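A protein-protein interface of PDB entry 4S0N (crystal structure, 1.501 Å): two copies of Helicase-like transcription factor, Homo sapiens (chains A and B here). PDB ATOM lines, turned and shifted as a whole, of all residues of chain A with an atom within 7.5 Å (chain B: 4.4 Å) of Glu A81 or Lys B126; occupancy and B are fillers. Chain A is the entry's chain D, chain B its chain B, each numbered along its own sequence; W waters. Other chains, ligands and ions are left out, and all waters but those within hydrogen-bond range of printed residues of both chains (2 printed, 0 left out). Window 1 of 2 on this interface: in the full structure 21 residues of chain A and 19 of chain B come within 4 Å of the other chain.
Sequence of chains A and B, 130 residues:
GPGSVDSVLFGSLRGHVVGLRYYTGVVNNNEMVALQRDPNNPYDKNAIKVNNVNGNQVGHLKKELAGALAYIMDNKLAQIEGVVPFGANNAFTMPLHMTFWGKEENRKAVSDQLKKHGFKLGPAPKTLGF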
ATOM      1  N   GLY A   1     -10.906 -18.894  21.635  1.00  0.00           N
ATOM      2  CA  GLY A   1     -10.464 -18.560  22.977  1.00  0.00           C
ATOM      3  C   GLY A   1     -10.262 -19.787  23.848  1.00  0.00           C
ATOM      4  O   GLY A   1     -10.495 -20.914  23.405  1.00  0.00           O
ATOM      5  N   PRO A   2      -9.825 -19.575  25.099  1.00  0.00           N
ATOM      6  CA  PRO A   2      -9.563 -20.670  26.040  1.00  0.00           C
ATOM      7  C   PRO A   2     -10.831 -21.422  26.432  1.00  0.00           C
ATOM      8  O   PRO A   2     -11.861 -20.806  26.715  1.00  0.00           O
ATOM      9  CB  PRO A   2      -8.951 -19.956  27.250  1.00  0.00           C
ATOM     10  CG  PRO A   2      -9.435 -18.551  27.149  1.00  0.00           C
ATOM     11  CD  PRO A   2      -9.525 -18.257  25.684  1.00  0.00           C
ATOM     12  N   GLY A   3     -10.749 -22.747  26.446  1.00  0.00           N
ATOM     13  CA  GLY A   3     -11.895 -23.569  26.783  1.00  0.00           C
ATOM     14  C   GLY A   3     -11.934 -23.942  28.250  1.00  0.00           C
ATOM     15  O   GLY A   3     -10.945 -23.796  28.966  1.00  0.00           O
ATOM     16  N   LEU A   9     -12.830 -33.135  22.988  1.00  0.00           N
ATOM     17  CA  LEU A   9     -12.845 -33.150  21.528  1.00  0.00           C
ATOM     18  C   LEU A   9     -14.222 -33.512  20.994  1.00  0.00           C
ATOM     19  O   LEU A   9     -14.806 -34.518  21.399  1.00  0.00           O
ATOM     20  CB  LEU A   9     -11.815 -34.144  20.990  1.00  0.00           C
ATOM     21  CG  LEU A   9     -10.362 -33.682  20.903  1.00  0.00           C
ATOM     22  CD1 LEU A   9      -9.446 -34.874  20.691  1.00  0.00           C
ATOM     23  CD2 LEU A   9     -10.203 -32.679  19.771  1.00  0.00           C
ATOM     24  N   LEU A  13     -13.092 -30.900  11.109  1.00  0.00           N
ATOM     25  CA  LEU A  13     -13.729 -30.391   9.892  1.00  0.00           C
ATOM     26  C   LEU A  13     -12.697 -29.760   8.957  1.00  0.00           C
ATOM     27  O   LEU A  13     -11.817 -29.038   9.417  1.00  0.00           O
ATOM     28  CB  LEU A  13     -14.783 -29.356  10.242  1.00  0.00           C
ATOM     29  CG  LEU A  13     -15.490 -28.693   9.060  1.00  0.00           C
ATOM     30  CD1 LEU A  13     -16.378 -29.693   8.328  1.00  0.00           C
ATOM     31  CD2 LEU A  13     -16.306 -27.509   9.546  1.00  0.00           C
ATOM     32  N   MET A  32      -0.878 -23.248  13.549  1.00  0.00           N
ATOM     33  CA  MET A  32      -2.138 -22.693  14.031  1.00  0.00           C
ATOM     34  C   MET A  32      -2.466 -21.397  13.343  1.00  0.00           C
ATOM     35  O   MET A  32      -1.572 -20.599  13.054  1.00  0.00           O
ATOM     36  CB  MET A  32      -2.068 -22.368  15.521  1.00  0.00           C
ATOM     37  CG  MET A  32      -2.250 -23.494  16.434  1.00  0.00           C
ATOM     38  SD  MET A  32      -2.516 -22.863  18.095  1.00  0.00           S
ATOM     39  CE  MET A  32      -0.968 -22.009  18.368  1.00  0.00           C
ATOM     40  N   VAL A  33      -3.755 -21.156  13.159  1.00  0.00           N
ATOM     41  CA  VAL A  33      -4.229 -19.828  12.831  1.00  0.00           C
ATOM     42  C   VAL A  33      -5.333 -19.485  13.814  1.00  0.00           C
ATOM     43  O   VAL A  33      -5.929 -20.380  14.427  1.00  0.00           O
ATOM     44  CB  VAL A  33      -4.738 -19.727  11.378  1.00  0.00           C
ATOM     45  CG1 VAL A  33      -3.571 -19.860  10.391  1.00  0.00           C
ATOM     46  CG2 VAL A  33      -5.816 -20.764  11.115  1.00  0.00           C
ATOM     47  N   ALA A  34      -5.603 -18.195  13.975  1.00  0.00           N
ATOM     48  CA  ALA A  34      -6.668 -17.757  14.860  1.00  0.00           C
ATOM     49  C   ALA A  34      -7.936 -17.494  14.064  1.00  0.00           C
ATOM     50  O   ALA A  34      -7.886 -16.847  13.016  1.00  0.00           O
ATOM     51  CB  ALA A  34      -6.255 -16.512  15.605  1.00  0.00           C
ATOM     52  N   LEU A  35      -9.069 -17.996  14.556  1.00  0.00           N
ATOM     53  CA  LEU A  35     -10.370 -17.644  14.002  1.00  0.00           C
ATOM     54  C   LEU A  35     -10.986 -16.559  14.860  1.00  0.00           C
ATOM     55  O   LEU A  35     -11.180 -16.737  16.063  1.00  0.00           O
ATOM     56  CB  LEU A  35     -11.298 -18.855  13.938  1.00  0.00           C
ATOM     57  CG  LEU A  35     -10.830 -20.077  13.142  1.00  0.00           C
ATOM     58  CD1 LEU A  35     -12.020 -20.961  12.833  1.00  0.00           C
ATOM     59  CD2 LEU A  35     -10.106 -19.670  11.875  1.00  0.00           C
ATOM     60  N   ALA A  78     -18.720 -24.110  21.100  1.00  0.00           N
ATOM     61  CA  ALA A  78     -17.457 -24.812  20.950  1.00  0.00           C
ATOM     62  C   ALA A  78     -16.329 -23.833  20.704  1.00  0.00           C
ATOM     63  O   ALA A  78     -16.545 -22.711  20.240  1.00  0.00           O
ATOM     64  CB  ALA A  78     -17.529 -25.820  19.806  1.00  0.00           C
ATOM     65  N   GLN A  79     -15.123 -24.267  21.042  1.00  0.00           N
ATOM     66  CA  GLN A  79     -13.919 -23.536  20.700  1.00  0.00           C
ATOM     67  C   GLN A  79     -13.319 -24.211  19.477  1.00  0.00           C
ATOM     68  O   GLN A  79     -13.249 -25.438  19.421  1.00  0.00           O
ATOM     69  CB  GLN A  79     -12.929 -23.521  21.871  1.00  0.00           C
ATOM     70  CG  GLN A  79     -13.431 -22.781  23.113  1.00  0.00           C
ATOM     71  CD  GLN A  79     -14.558 -23.509  23.834  1.00  0.00           C
ATOM     72  OE1 GLN A  79     -15.630 -22.947  24.060  1.00  0.00           O
ATOM     73  NE2 GLN A  79     -14.317 -24.762  24.201  1.00  0.00           N
ATOM     74  N   ILE A  80     -12.903 -23.420  18.499  1.00  0.00           N
ATOM     75  CA  ILE A  80     -12.412 -23.975  17.245  1.00  0.00           C
ATOM     76  C   ILE A  80     -10.943 -23.645  17.047  1.00  0.00           C
ATOM     77  O   ILE A  80     -10.551 -22.477  17.105  1.00  0.00           O
ATOM     78  CB  ILE A  80     -13.226 -23.443  16.059  1.00  0.00           C
ATOM     79  CG1 ILE A  80     -14.727 -23.545  16.359  1.00  0.00           C
ATOM     80  CG2 ILE A  80     -12.869 -24.197  14.784  1.00  0.00           C
ATOM     81  CD1 ILE A  80     -15.614 -22.925  15.295  1.00  0.00           C
ATOM     82  N   GLU A  81     -10.127 -24.675  16.840  1.00  0.00           N
ATOM     83  CA  GLU A  81      -8.715 -24.465  16.561  1.00  0.00           C
ATOM     84  C   GLU A  81      -8.492 -24.706  15.077  1.00  0.00           C
ATOM     85  O   GLU A  81      -8.892 -25.739  14.551  1.00  0.00           O
ATOM     86  CB  GLU A  81      -7.816 -25.390  17.401  1.00  0.00           C
ATOM     87  CG  GLU A  81      -6.315 -25.258  17.070  1.00  0.00           C
ATOM     88  CD  GLU A  81      -5.426 -26.345  17.701  1.00  0.00           C
ATOM     89  OE1 GLU A  81      -5.467 -27.522  17.249  1.00  0.00           O
ATOM     90  OE2 GLU A  81      -4.661 -26.014  18.629  1.00  0.00           O
ATOM     91  N   GLY A  82      -7.867 -23.749  14.406  1.00  0.00           N
ATOM     92  CA  GLY A  82      -7.571 -23.878  12.992  1.00  0.00           C
ATOM     93  C   GLY A  82      -6.096 -24.171  12.763  1.00  0.00           C
ATOM     94  O   GLY A  82      -5.235 -23.710  13.516  1.00  0.00           O
ATOM     95  N   VAL A  83      -5.814 -24.966  11.736  1.00  0.00           N
ATOM     96  CA  VAL A  83      -4.455 -25.291  11.325  1.00  0.00           C
ATOM     97  C   VAL A  83      -4.418 -25.326   9.813  1.00  0.00           C
ATOM     98  O   VAL A  83      -5.302 -25.910   9.190  1.00  0.00           O
ATOM     99  CB  VAL A  83      -3.986 -26.668  11.868  1.00  0.00           C
ATOM    100  CG1 VAL A  83      -2.611 -27.044  11.299  1.00  0.00           C
ATOM    101  CG2 VAL A  83      -3.978 -26.676  13.381  1.00  0.00           C
ATOM    102  N   LEU A  96      -7.872 -25.422   5.283  1.00  0.00           N
ATOM    103  CA  LEU A  96      -7.862 -25.228   6.715  1.00  0.00           C
ATOM    104  C   LEU A  96      -8.440 -26.458   7.402  1.00  0.00           C
ATOM    105  O   LEU A  96      -9.491 -26.972   6.996  1.00  0.00           O
ATOM    106  CB  LEU A  96      -8.672 -23.982   7.081  1.00  0.00           C
ATOM    107  CG  LEU A  96      -8.700 -23.658   8.564  1.00  0.00           C
ATOM    108  CD1 LEU A  96      -7.329 -23.164   8.969  1.00  0.00           C
ATOM    109  CD2 LEU A  96      -9.763 -22.629   8.887  1.00  0.00           C
ATOM    110  N   HIS A  97      -7.747 -26.942   8.426  1.00  0.00           N
ATOM    111  CA  HIS A  97      -8.257 -28.043   9.239  1.00  0.00           C
ATOM    112  C   HIS A  97      -8.726 -27.474  10.566  1.00  0.00           C
ATOM    113  O   HIS A  97      -7.992 -26.737  11.211  1.00  0.00           O
ATOM    114  CB  HIS A  97      -7.178 -29.112   9.472  1.00  0.00           C
ATOM    115  CG  HIS A  97      -6.927 -30.004   8.293  1.00  0.00           C
ATOM    116  ND1 HIS A  97      -5.871 -30.890   8.245  1.00  0.00           N
ATOM    117  CD2 HIS A  97      -7.589 -30.146   7.120  1.00  0.00           C
ATOM    118  CE1 HIS A  97      -5.899 -31.546   7.097  1.00  0.00           C
ATOM    119  NE2 HIS A  97      -6.931 -31.113   6.396  1.00  0.00           N
ATOM    120  N   MET A  98      -9.943 -27.809  10.975  1.00  0.00           N
ATOM    121  CA  MET A  98     -10.480 -27.304  12.225  1.00  0.00           C
ATOM    122  C   MET A  98     -10.789 -28.430  13.205  1.00  0.00           C
ATOM    123  O   MET A  98     -11.336 -29.458  12.817  1.00  0.00           O
ATOM    124  CB  MET A  98     -11.742 -26.490  11.956  1.00  0.00           C
ATOM    125  CG  MET A  98     -11.483 -25.213  11.190  1.00  0.00           C
ATOM    126  SD  MET A  98     -12.953 -24.636  10.332  1.00  0.00           S
ATOM    127  CE  MET A  98     -12.924 -25.685   8.875  1.00  0.00           C
ATOM    128  N   THR A  99     -10.435 -28.238  14.469  1.00  0.00           N
ATOM    129  CA  THR A  99     -10.849 -29.169  15.509  1.00  0.00           C
ATOM    130  C   THR A  99     -11.768 -28.450  16.487  1.00  0.00           C
ATOM    131  O   THR A  99     -11.547 -27.286  16.833  1.00  0.00           O
ATOM    132  CB  THR A  99      -9.648 -29.784  16.257  1.00  0.00           C
ATOM    133  OG1 THR A  99      -8.834 -28.744  16.804  1.00  0.00           O
ATOM    134  CG2 THR A  99      -8.802 -30.620  15.311  1.00  0.00           C
ATOM    135  N   PHE A 100     -12.812 -29.148  16.916  1.00  0.00           N
ATOM    136  CA  PHE A 100     -13.832 -28.569  17.777  1.00  0.00           C
ATOM    137  C   PHE A 100     -13.725 -29.109  19.197  1.00  0.00           C
ATOM    138  O   PHE A 100     -13.700 -30.324  19.411  1.00  0.00           O
ATOM    139  CB  PHE A 100     -15.232 -28.852  17.214  1.00  0.00           C
ATOM    140  CG  PHE A 100     -15.561 -28.068  15.969  1.00  0.00           C
ATOM    141  CD1 PHE A 100     -14.902 -28.318  14.771  1.00  0.00           C
ATOM    142  CD2 PHE A 100     -16.536 -27.083  15.994  1.00  0.00           C
ATOM    143  CE1 PHE A 100     -15.208 -27.596  13.629  1.00  0.00           C
ATOM    144  CE2 PHE A 100     -16.846 -26.359  14.854  1.00  0.00           C
ATOM    145  CZ  PHE A 100     -16.182 -26.615  13.673  1.00  0.00           C
ATOM    146  N   TRP A 101     -13.653 -28.194  20.158  1.00  0.00           N
ATOM    147  CA  TRP A 101     -13.627 -28.543  21.573  1.00  0.00           C
ATOM    148  C   TRP A 101     -14.826 -27.950  22.292  1.00  0.00           C
ATOM    149  O   TRP A 101     -15.262 -26.844  21.976  1.00  0.00           O
ATOM    150  CB  TRP A 101     -12.349 -28.032  22.238  1.00  0.00           C
ATOM    151  CG  TRP A 101     -11.092 -28.731  21.836  1.00  0.00           C
ATOM    152  CD1 TRP A 101     -10.375 -28.540  20.689  1.00  0.00           C
ATOM    153  CD2 TRP A 101     -10.377 -29.709  22.601  1.00  0.00           C
ATOM    154  NE1 TRP A 101      -9.265 -29.352  20.686  1.00  0.00           N
ATOM    155  CE2 TRP A 101      -9.245 -30.079  21.849  1.00  0.00           C
ATOM    156  CE3 TRP A 101     -10.591 -30.316  23.844  1.00  0.00           C
ATOM    157  CZ2 TRP A 101      -8.325 -31.026  22.301  1.00  0.00           C
ATOM    158  CZ3 TRP A 101      -9.677 -31.251  24.293  1.00  0.00           C
ATOM    159  CH2 TRP A 101      -8.558 -31.600  23.520  1.00  0.00           C
ATOM    160  N   GLU B  81      -4.121 -22.182  28.566  1.00  0.00           N
ATOM    161  CA  GLU B  81      -4.899 -23.406  28.450  1.00  0.00           C
ATOM    162  C   GLU B  81      -3.948 -24.577  28.315  1.00  0.00           C
ATOM    163  O   GLU B  81      -3.102 -24.580  27.432  1.00  0.00           O
ATOM    164  CB  GLU B  81      -5.817 -23.315  27.230  1.00  0.00           C
ATOM    165  CG  GLU B  81      -6.674 -24.517  26.925  1.00  0.00           C
ATOM    166  CD  GLU B  81      -7.465 -24.296  25.641  1.00  0.00           C
ATOM    167  OE1 GLU B  81      -6.960 -23.575  24.749  1.00  0.00           O
ATOM    168  OE2 GLU B  81      -8.594 -24.813  25.530  1.00  0.00           O
ATOM    169  N   VAL B  83      -3.260 -28.746  27.848  1.00  0.00           N
ATOM    170  CA  VAL B  83      -3.785 -30.045  27.463  1.00  0.00           C
ATOM    171  C   VAL B  83      -2.641 -31.051  27.456  1.00  0.00           C
ATOM    172  O   VAL B  83      -1.486 -30.694  27.196  1.00  0.00           O
ATOM    173  CB  VAL B  83      -4.496 -29.989  26.078  1.00  0.00           C
ATOM    174  CG1 VAL B  83      -3.500 -29.725  24.958  1.00  0.00           C
ATOM    175  CG2 VAL B  83      -5.286 -31.269  25.821  1.00  0.00           C
ATOM    176  N   HIS B  97       0.944 -29.300  26.572  1.00  0.00           N
ATOM    177  CA  HIS B  97       0.835 -28.299  25.520  1.00  0.00           C
ATOM    178  C   HIS B  97       0.035 -27.123  26.063  1.00  0.00           C
ATOM    179  O   HIS B  97      -1.082 -27.294  26.559  1.00  0.00           O
ATOM    180  CB  HIS B  97       0.171 -28.886  24.269  1.00  0.00           C
ATOM    181  CG  HIS B  97      -0.052 -27.886  23.179  1.00  0.00           C
ATOM    182  ND1 HIS B  97       0.785 -27.770  22.090  1.00  0.00           N
ATOM    183  CD2 HIS B  97      -1.008 -26.940  23.019  1.00  0.00           C
ATOM    184  CE1 HIS B  97       0.345 -26.808  21.298  1.00  0.00           C
ATOM    185  NE2 HIS B  97      -0.739 -26.287  21.842  1.00  0.00           N
ATOM    186  N   THR B  99      -1.587 -23.258  25.419  1.00  0.00           N
ATOM    187  CA  THR B  99      -1.991 -22.241  24.467  1.00  0.00           C
ATOM    188  C   THR B  99      -2.277 -20.948  25.221  1.00  0.00           C
ATOM    189  O   THR B  99      -2.964 -20.952  26.247  1.00  0.00           O
ATOM    190  CB  THR B  99      -3.234 -22.669  23.660  1.00  0.00           C
ATOM    191  OG1 THR B  99      -3.013 -23.969  23.091  1.00  0.00           O
ATOM    192  CG2 THR B  99      -3.504 -21.687  22.537  1.00  0.00           C
ATOM    193  N   ALA B 124       2.683 -24.031  17.047  1.00  0.00           N
ATOM    194  CA  ALA B 124       2.305 -25.447  17.080  1.00  0.00           C
ATOM    195  C   ALA B 124       0.905 -25.625  17.666  1.00  0.00           C
ATOM    196  O   ALA B 124       0.596 -25.119  18.746  1.00  0.00           O
ATOM    197  CB  ALA B 124       3.314 -26.249  17.873  1.00  0.00           C
ATOM    198  N   PRO B 125       0.047 -26.351  16.955  1.00  0.00           N
ATOM    199  CA  PRO B 125      -1.305 -26.596  17.472  1.00  0.00           C
ATOM    200  C   PRO B 125      -1.349 -27.708  18.514  1.00  0.00           C
ATOM    201  O   PRO B 125      -0.367 -28.428  18.687  1.00  0.00           O
ATOM    202  CB  PRO B 125      -2.078 -27.009  16.226  1.00  0.00           C
ATOM    203  CG  PRO B 125      -1.039 -27.710  15.382  1.00  0.00           C
ATOM    204  CD  PRO B 125       0.237 -26.921  15.608  1.00  0.00           C
ATOM    205  N   LYS B 126      -2.491 -27.844  19.180  1.00  0.00           N
ATOM    206  CA  LYS B 126      -2.722 -28.951  20.095  1.00  0.00           C
ATOM    207  C   LYS B 126      -2.569 -30.276  19.367  1.00  0.00           C
ATOM    208  O   LYS B 126      -2.077 -31.252  19.933  1.00  0.00           O
ATOM    209  CB  LYS B 126      -4.115 -28.870  20.707  1.00  0.00           C
ATOM    210  CG  LYS B 126      -4.325 -27.738  21.669  1.00  0.00           C
ATOM    211  CD  LYS B 126      -5.716 -27.817  22.282  1.00  0.00           C
ATOM    212  CE  LYS B 126      -6.542 -26.578  21.968  1.00  0.00           C
ATOM    213  NZ  LYS B 126      -5.913 -25.331  22.496  1.00  0.00           N
ATOM    214  N   THR B 127      -3.017 -30.309  18.114  1.00  0.00           N
ATOM    215  CA  THR B 127      -2.844 -31.487  17.271  1.00  0.00           C
ATOM    216  C   THR B 127      -2.639 -31.106  15.807  1.00  0.00           C
ATOM    217  O   THR B 127      -3.199 -30.119  15.320  1.00  0.00           O
ATOM    218  CB  THR B 127      -4.050 -32.433  17.372  1.00  0.00           C
ATOM    219  OG1 THR B 127      -3.826 -33.569  16.532  1.00  0.00           O
ATOM    220  CG2 THR B 127      -5.324 -31.734  16.922  1.00  0.00           C
HETATM  221  O   HOH W   1      -2.407 -24.627  20.510  1.00  0.00           O
HETATM  222  O   HOH W   2      -4.950 -24.368  20.368  1.00  0.00           O
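Met A32 touches Ala B124. Met A32 touches Pro B125. OE1 of Glu A81 touches CB of Pro B125 (3.6 Å). N of Thr B127 touches OE1 of Glu A81, 3.8 Å away. Pro B125 touches Val A83 (CB to CG2, 3.4 Å). Thr B127 touches Thr A99.
Of the 21 printed residues of chain A, 5 touch a printed residue of chain B. Of the 8 printed residues of chain B, 5 touch a printed residue of chain A. Along chain B the printed residues that touch a printed residue of chain A span positions 81 to 127. Among the printed residues, 8 pairs touch across the chains. Among the printed residues, no Asp or Glu carboxylate lies within 4 Å of a Lys or Arg side-chain nitrogen of the other chain.
Water W2 lies within hydrogen-bond range of OE2 of Glu A81 (2.4 Å), NZ of Lys B126 (2.5 Å), OG1 of Thr B99 (3.4 Å) and SD of Met A32 (3.7 Å). Water W1 lies within hydrogen-bond range of a ring nitrogen (NE2) of His B97, the side-chain hydroxyl (OG1) of Thr B99, the side-chain sulfur (SD) of Met A32, the side-chain carboxylate (OE2) of Glu A81 and the backbone NH (N) of Lys B126.
Printed residues of chain B within 4 Å of Glu A81: Pro B125 (3.6 Å), Lys B126 (2.9 Å) and Thr B127 (3.8 Å). Printed residues of chain A within 4 Å of Lys B126: Glu A81. Printed residues of chain A within 4 Å of Glu B81: Gly A3 (3.1 Å). Of the printed residues of chain A, Pro B125 touches Met A32 (3.4 Å), Glu A81 (3.6 Å) and Val A83 (3.4 Å). His A97 touches none of the printed residues of chain B. The nearest printed residue of chain B that does not touch Glu A81 is His B97 (5.1 Å). The nearest residue of chain A that does not touch Lys B126 is Trp A101 (4.1 Å).
The side-chain carboxylate (OE2) of Glu B81 sits at hydrogen-bond distance from the backbone NH (N) of Gly A3 (3.1 Å). OE2 of Glu A81 is in hydrogen-bond range of N of Lys B126 (2.9 Å).
The backbone NH (N) of Thr B99 sits at hydrogen-bond distance from the backbone carbonyl oxygen (O) of Glu B81, 2.8 Å away. OE1 of Glu B81 lies within salt-bridge range of NZ of Lys B126, 3.0 Å away. OG1 of Thr B99 is in hydrogen-bond range of NZ of Lys B126, at 3.3 Å. The backbone NH (N) of Thr A99 lies within hydrogen-bond range of the backbone carbonyl oxygen (O) of Glu A81, 2.9 Å away. The backbone carbonyl oxygen (O) of Val A83 is in hydrogen-bond range of the backbone NH (N) of His A97 (2.8 Å).
4 positions are printed for both chains. Of the 8 pairs that touch across the chains among the printed residues, none has its exchanged pair printed and touching as well.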
